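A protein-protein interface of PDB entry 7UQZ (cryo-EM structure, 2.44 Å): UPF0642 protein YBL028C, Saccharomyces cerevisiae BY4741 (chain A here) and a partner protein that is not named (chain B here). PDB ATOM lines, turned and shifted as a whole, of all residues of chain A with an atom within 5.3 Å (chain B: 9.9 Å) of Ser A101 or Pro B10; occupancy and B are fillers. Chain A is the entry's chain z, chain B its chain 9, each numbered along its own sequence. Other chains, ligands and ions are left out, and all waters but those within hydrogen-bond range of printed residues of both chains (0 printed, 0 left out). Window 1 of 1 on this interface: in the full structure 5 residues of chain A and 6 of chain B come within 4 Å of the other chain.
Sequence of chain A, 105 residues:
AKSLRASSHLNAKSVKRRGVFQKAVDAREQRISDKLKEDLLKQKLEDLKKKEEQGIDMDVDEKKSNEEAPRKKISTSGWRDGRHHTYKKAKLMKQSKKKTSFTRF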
ATOM      1  N   GLN A  95      15.910   9.009  -5.403  1.00  0.00           N
ATOM      2  CA  GLN A  95      15.470   8.893  -6.791  1.00  0.00           C
ATOM      3  C   GLN A  95      16.649   8.959  -7.755  1.00  0.00           C
ATOM      4  O   GLN A  95      16.682   8.229  -8.751  1.00  0.00           O
ATOM      5  CB  GLN A  95      14.447   9.978  -7.119  1.00  0.00           C
ATOM      6  CG  GLN A  95      13.104   9.776  -6.443  1.00  0.00           C
ATOM      7  CD  GLN A  95      12.074  10.792  -6.886  1.00  0.00           C
ATOM      8  OE1 GLN A  95      12.242  11.460  -7.903  1.00  0.00           O
ATOM      9  NE2 GLN A  95      10.999  10.912  -6.119  1.00  0.00           N
ATOM     10  N   LYS A  99      17.474   5.740 -10.006  1.00  0.00           N
ATOM     11  CA  LYS A  99      17.090   6.053 -11.387  1.00  0.00           C
ATOM     12  C   LYS A  99      15.584   5.895 -11.600  1.00  0.00           C
ATOM     13  O   LYS A  99      15.128   5.325 -12.594  1.00  0.00           O
ATOM     14  CB  LYS A  99      17.881   5.203 -12.386  1.00  0.00           C
ATOM     15  CG  LYS A  99      19.372   5.476 -12.386  1.00  0.00           C
ATOM     16  CD  LYS A  99      20.124   4.448 -13.213  1.00  0.00           C
ATOM     17  CE  LYS A  99      21.597   4.807 -13.327  1.00  0.00           C
ATOM     18  NZ  LYS A  99      22.222   5.002 -11.991  1.00  0.00           N
ATOM     19  N   THR A 100      14.806   6.414 -10.655  1.00  0.00           N
ATOM     20  CA  THR A 100      13.349   6.358 -10.699  1.00  0.00           C
ATOM     21  C   THR A 100      12.742   7.757 -10.687  1.00  0.00           C
ATOM     22  O   THR A 100      11.704   7.997 -10.068  1.00  0.00           O
ATOM     23  CB  THR A 100      12.798   5.531  -9.540  1.00  0.00           C
ATOM     24  OG1 THR A 100      13.202   6.117  -8.297  1.00  0.00           O
ATOM     25  CG2 THR A 100      13.310   4.097  -9.612  1.00  0.00           C
ATOM     26  N   SER A 101      13.377   8.698 -11.378  1.00  0.00           N
ATOM     27  CA  SER A 101      12.928  10.082 -11.407  1.00  0.00           C
ATOM     28  C   SER A 101      12.137  10.360 -12.679  1.00  0.00           C
ATOM     29  O   SER A 101      12.493   9.887 -13.761  1.00  0.00           O
ATOM     30  CB  SER A 101      14.113  11.043 -11.309  1.00  0.00           C
ATOM     31  OG  SER A 101      13.675  12.389 -11.331  1.00  0.00           O
ATOM     32  N   PHE A 102      11.057  11.132 -12.539  1.00  0.00           N
ATOM     33  CA  PHE A 102      10.214  11.459 -13.683  1.00  0.00           C
ATOM     34  C   PHE A 102      10.852  12.504 -14.592  1.00  0.00           C
ATOM     35  O   PHE A 102      10.718  12.421 -15.818  1.00  0.00           O
ATOM     36  CB  PHE A 102       8.845  11.950 -13.205  1.00  0.00           C
ATOM     37  CG  PHE A 102       7.884  10.846 -12.871  1.00  0.00           C
ATOM     38  CD1 PHE A 102       7.823  10.322 -11.591  1.00  0.00           C
ATOM     39  CD2 PHE A 102       7.032  10.339 -13.837  1.00  0.00           C
ATOM     40  CE1 PHE A 102       6.932   9.310 -11.281  1.00  0.00           C
ATOM     41  CE2 PHE A 102       6.142   9.327 -13.534  1.00  0.00           C
ATOM     42  CZ  PHE A 102       6.092   8.812 -12.255  1.00  0.00           C
ATOM     43  N   THR A 103      11.550  13.489 -14.024  1.00  0.00           N
ATOM     44  CA  THR A 103      12.018  14.636 -14.791  1.00  0.00           C
ATOM     45  C   THR A 103      13.528  14.749 -14.929  1.00  0.00           C
ATOM     46  O   THR A 103      13.988  15.508 -15.787  1.00  0.00           O
ATOM     47  CB  THR A 103      11.505  15.945 -14.171  1.00  0.00           C
ATOM     48  OG1 THR A 103      11.795  15.956 -12.769  1.00  0.00           O
ATOM     49  CG2 THR A 103      10.013  16.088 -14.383  1.00  0.00           C
ATOM     50  N   ARG A 104      14.309  14.038 -14.123  1.00  0.00           N
ATOM     51  CA  ARG A 104      15.759  14.169 -14.131  1.00  0.00           C
ATOM     52  C   ARG A 104      16.405  12.822 -14.409  1.00  0.00           C
ATOM     53  O   ARG A 104      15.961  11.791 -13.894  1.00  0.00           O
ATOM     54  CB  ARG A 104      16.266  14.728 -12.796  1.00  0.00           C
ATOM     55  CG  ARG A 104      15.741  16.114 -12.468  1.00  0.00           C
ATOM     56  CD  ARG A 104      16.077  16.515 -11.044  1.00  0.00           C
ATOM     57  NE  ARG A 104      15.731  17.906 -10.776  1.00  0.00           N
ATOM     58  CZ  ARG A 104      16.560  18.928 -10.938  1.00  0.00           C
ATOM     59  NH1 ARG A 104      17.800  18.751 -11.364  1.00  0.00           N
ATOM     60  NH2 ARG A 104      16.135  20.157 -10.667  1.00  0.00           N
ATOM     61  N   PRO B   2       9.263   0.818 -20.263  1.00  0.00           N
ATOM     62  CA  PRO B   2       8.569   1.603 -19.235  1.00  0.00           C
ATOM     63  C   PRO B   2       7.066   1.341 -19.209  1.00  0.00           C
ATOM     64  O   PRO B   2       6.498   0.919 -20.214  1.00  0.00           O
ATOM     65  CB  PRO B   2       8.863   3.049 -19.644  1.00  0.00           C
ATOM     66  CG  PRO B   2       9.100   2.982 -21.111  1.00  0.00           C
ATOM     67  CD  PRO B   2       9.771   1.663 -21.357  1.00  0.00           C
ATOM     68  N   SER B   3       6.440   1.582 -18.061  1.00  0.00           N
ATOM     69  CA  SER B   3       5.005   1.380 -17.929  1.00  0.00           C
ATOM     70  C   SER B   3       4.233   2.453 -18.687  1.00  0.00           C
ATOM     71  O   SER B   3       4.678   3.595 -18.820  1.00  0.00           O
ATOM     72  CB  SER B   3       4.599   1.390 -16.456  1.00  0.00           C
ATOM     73  OG  SER B   3       3.199   1.238 -16.309  1.00  0.00           O
ATOM     74  N   SER B   6       3.358   5.480 -16.569  1.00  0.00           N
ATOM     75  CA  SER B   6       4.430   6.425 -16.264  1.00  0.00           C
ATOM     76  C   SER B   6       5.539   6.205 -17.290  1.00  0.00           C
ATOM     77  O   SER B   6       6.391   5.331 -17.105  1.00  0.00           O
ATOM     78  CB  SER B   6       4.935   6.239 -14.841  1.00  0.00           C
ATOM     79  OG  SER B   6       5.285   4.889 -14.598  1.00  0.00           O
ATOM     80  N   ILE B   7       5.527   7.002 -18.355  1.00  0.00           N
ATOM     81  CA  ILE B   7       6.502   6.825 -19.424  1.00  0.00           C
ATOM     82  C   ILE B   7       7.796   7.591 -19.161  1.00  0.00           C
ATOM     83  O   ILE B   7       8.850   7.215 -19.683  1.00  0.00           O
ATOM     84  CB  ILE B   7       5.891   7.232 -20.776  1.00  0.00           C
ATOM     85  CG1 ILE B   7       5.363   8.665 -20.709  1.00  0.00           C
ATOM     86  CG2 ILE B   7       4.788   6.266 -21.172  1.00  0.00           C
ATOM     87  CD1 ILE B   7       4.941   9.214 -22.042  1.00  0.00           C
ATOM     88  N   ASN B   8       7.745   8.651 -18.357  1.00  0.00           N
ATOM     89  CA  ASN B   8       8.923   9.466 -18.088  1.00  0.00           C
ATOM     90  C   ASN B   8       9.788   8.910 -16.966  1.00  0.00           C
ATOM     91  O   ASN B   8      10.807   9.524 -16.633  1.00  0.00           O
ATOM     92  CB  ASN B   8       8.506  10.902 -17.758  1.00  0.00           C
ATOM     93  CG  ASN B   8       7.924  11.631 -18.954  1.00  0.00           C
ATOM     94  OD1 ASN B   8       8.269  11.342 -20.098  1.00  0.00           O
ATOM     95  ND2 ASN B   8       7.037  12.582 -18.692  1.00  0.00           N
ATOM     96  N   ARG B   9       9.409   7.782 -16.368  1.00  0.00           N
ATOM     97  CA  ARG B   9      10.197   7.160 -15.318  1.00  0.00           C
ATOM     98  C   ARG B   9      10.792   5.852 -15.810  1.00  0.00           C
ATOM     99  O   ARG B   9      10.050   4.979 -16.277  1.00  0.00           O
ATOM    100  CB  ARG B   9       9.341   6.905 -14.073  1.00  0.00           C
ATOM    101  CG  ARG B   9      10.128   6.349 -12.900  1.00  0.00           C
ATOM    102  CD  ARG B   9       9.306   6.353 -11.630  1.00  0.00           C
ATOM    103  NE  ARG B   9       8.160   5.457 -11.710  1.00  0.00           N
ATOM    104  CZ  ARG B   9       7.243   5.337 -10.762  1.00  0.00           C
ATOM    105  NH1 ARG B   9       7.300   6.053  -9.652  1.00  0.00           N
ATOM    106  NH2 ARG B   9       6.242   4.478 -10.934  1.00  0.00           N
ATOM    107  N   PRO B  10      12.113   5.686 -15.742  1.00  0.00           N
ATOM    108  CA  PRO B  10      12.715   4.410 -16.151  1.00  0.00           C
ATOM    109  C   PRO B  10      12.308   3.273 -15.224  1.00  0.00           C
ATOM    110  O   PRO B  10      12.271   3.423 -14.001  1.00  0.00           O
ATOM    111  CB  PRO B  10      14.222   4.684 -16.068  1.00  0.00           C
ATOM    112  CG  PRO B  10      14.348   6.175 -16.094  1.00  0.00           C
ATOM    113  CD  PRO B  10      13.129   6.692 -15.400  1.00  0.00           C
ATOM    114  N   LYS B  11      11.994   2.128 -15.828  1.00  0.00           N
ATOM    115  CA  LYS B  11      11.567   0.946 -15.088  1.00  0.00           C
ATOM    116  C   LYS B  11      12.531  -0.220 -15.270  1.00  0.00           C
ATOM    117  O   LYS B  11      13.083  -0.725 -14.283  1.00  0.00           O
ATOM    118  CB  LYS B  11      10.148   0.573 -15.539  1.00  0.00           C
ATOM    119  CG  LYS B  11       9.468  -0.523 -14.748  1.00  0.00           C
ATOM    120  CD  LYS B  11       8.051  -0.719 -15.263  1.00  0.00           C
ATOM    121  CE  LYS B  11       7.339  -1.852 -14.552  1.00  0.00           C
ATOM    122  NZ  LYS B  11       7.252  -1.631 -13.085  1.00  0.00           N
ATOM    123  N   LEU B  12      12.768  -0.645 -16.514  1.00  0.00           N
ATOM    124  CA  LEU B  12      13.623  -1.801 -16.766  1.00  0.00           C
ATOM    125  C   LEU B  12      15.070  -1.522 -16.382  1.00  0.00           C
ATOM    126  O   LEU B  12      15.733  -2.379 -15.786  1.00  0.00           O
ATOM    127  CB  LEU B  12      13.530  -2.210 -18.235  1.00  0.00           C
ATOM    128  CG  LEU B  12      14.514  -3.290 -18.691  1.00  0.00           C
ATOM    129  CD1 LEU B  12      14.139  -4.642 -18.109  1.00  0.00           C
ATOM    130  CD2 LEU B  12      14.596  -3.354 -20.203  1.00  0.00           C
ATOM    131  N   THR B  13      15.580  -0.335 -16.722  1.00  0.00           N
ATOM    132  CA  THR B  13      16.963  -0.004 -16.397  1.00  0.00           C
ATOM    133  C   THR B  13      17.177   0.071 -14.891  1.00  0.00           C
ATOM    134  O   THR B  13      18.200  -0.399 -14.382  1.00  0.00           O
ATOM    135  CB  THR B  13      17.364   1.313 -17.062  1.00  0.00           C
ATOM    136  OG1 THR B  13      16.388   2.319 -16.768  1.00  0.00           O
ATOM    137  CG2 THR B  13      17.465   1.140 -18.567  1.00  0.00           C
ATOM    138  N   SER B  14      16.222   0.656 -14.164  1.00  0.00           N
ATOM    139  CA  SER B  14      16.324   0.706 -12.709  1.00  0.00           C
ATOM    140  C   SER B  14      16.277  -0.690 -12.100  1.00  0.00           C
ATOM    141  O   SER B  14      17.034  -0.995 -11.166  1.00  0.00           O
ATOM    142  CB  SER B  14      15.209   1.580 -12.138  1.00  0.00           C
ATOM    143  OG  SER B  14      13.936   1.039 -12.437  1.00  0.00           O
ATOM    144  N   ASN B  15      15.397  -1.556 -12.619  1.00  0.00           N
ATOM    145  CA  ASN B  15      15.340  -2.932 -12.132  1.00  0.00           C
ATOM    146  C   ASN B  15      16.653  -3.664 -12.382  1.00  0.00           C
ATOM    147  O   ASN B  15      17.142  -4.389 -11.507  1.00  0.00           O
ATOM    148  CB  ASN B  15      14.179  -3.678 -12.790  1.00  0.00           C
ATOM    149  CG  ASN B  15      12.831  -3.189 -12.315  1.00  0.00           C
ATOM    150  OD1 ASN B  15      12.679  -2.775 -11.169  1.00  0.00           O
ATOM    151  ND2 ASN B  15      11.838  -3.237 -13.197  1.00  0.00           N
ATOM    152  N   LEU B  16      17.241  -3.480 -13.568  1.00  0.00           N
ATOM    153  CA  LEU B  16      18.521  -4.111 -13.873  1.00  0.00           C
ATOM    154  C   LEU B  16      19.631  -3.584 -12.974  1.00  0.00           C
ATOM    155  O   LEU B  16      20.498  -4.349 -12.536  1.00  0.00           O
ATOM    156  CB  LEU B  16      18.887  -3.891 -15.340  1.00  0.00           C
ATOM    157  CG  LEU B  16      18.073  -4.604 -16.418  1.00  0.00           C
ATOM    158  CD1 LEU B  16      18.701  -4.369 -17.782  1.00  0.00           C
ATOM    159  CD2 LEU B  16      17.968  -6.089 -16.121  1.00  0.00           C
ATOM    160  N   HIS B  17      19.635  -2.276 -12.709  1.00  0.00           N
ATOM    161  CA  HIS B  17      20.646  -1.686 -11.837  1.00  0.00           C
ATOM    162  C   HIS B  17      20.555  -2.266 -10.431  1.00  0.00           C
ATOM    163  O   HIS B  17      21.572  -2.648  -9.832  1.00  0.00           O
ATOM    164  CB  HIS B  17      20.474  -0.166 -11.814  1.00  0.00           C
ATOM    165  CG  HIS B  17      21.540   0.558 -11.055  1.00  0.00           C
ATOM    166  ND1 HIS B  17      22.769   0.860 -11.603  1.00  0.00           N
ATOM    167  CD2 HIS B  17      21.561   1.048  -9.794  1.00  0.00           C
ATOM    168  CE1 HIS B  17      23.500   1.502 -10.710  1.00  0.00           C
ATOM    169  NE2 HIS B  17      22.791   1.628  -9.603  1.00  0.00           N
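The backbone carbonyl oxygen (O) of Ser A101 lies close to the backbone carbonyl oxygen (O) of Asn B8 (3.4 Å).
The backbone carbonyl oxygen of Phe A102 lies close to the backbone carbonyl oxygen of Asn B8 (3.0 Å).
The backbone carbonyl oxygen of Gln A95 is in hydrogen-bond range of the backbone NH of Thr A100.
OG of Ser B14 sits at hydrogen-bond distance from O of Pro B10 (3.3 Å).
O of Lys B11 is in hydrogen-bond range of OG of Ser B14 (2.7 Å).
N of Arg A104 lies within hydrogen-bond range of OG of Ser A101, at 3.3 Å.
Pro B10 touches Lys A99.
CB of Ser B14 touches O of Lys A99 (3.8 Å).
Lys A99 touches His B17.
Thr A100 touches Arg B9.
O of Ser A101 touches CA of Arg B9, at 3.9 Å.
CD of Pro B10 touches O of Ser A101, 3.6 Å away.
CB of Ser B6 touches CE2 of Phe A102 (3.6 Å).
CE1 of Phe A102 touches NH1 of Arg B9, at 3.7 Å.
Gln A95 touches none of the printed residues of chain B.
Of the printed residues of chain B, Lys A99 touches Pro B10, Ser B14 and His B17.
Of chain B, only Arg B9 comes within 4 Å of Thr A100.
Of chain B, only Asn B8, Arg B9 and Pro B10 come within 4 Å of Ser A101.
Printed residues of chain B within 4 Å of Phe A102: Ser B6, Asn B8 and Arg B9.
Arg A104 touches none of the printed residues of chain B.
Printed residues of chain A within 4 Å of Ser B6: Phe A102.
Of the printed residues of chain A, Asn B8 touches Ser A101 (3.4 Å) and Phe A102 (3.0 Å).
Of chain A, only Lys A99 and Ser A101 come within 4 Å of Pro B10.
Printed residues of chain A within 4 Å of Ser B14: Lys A99.
The nearest printed residue of chain A that does not touch Asn B8 is Thr A103 (4.8 Å).
Of the 7 printed residues of chain A, 4 touch a printed residue of chain B.
Hydrophobic or aromatic side chains of chain A within 4 Å of the printed part of chain B: Phe A102.
Printed residues of chain B that touch a printed residue of chain A: Ser B6, Asn B8, Arg B9, Pro B10, Ser B14 and His B17.
Hydrophobic or aromatic side chains of chain B that line the printed part of chain A: Pro B10 and His B17.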
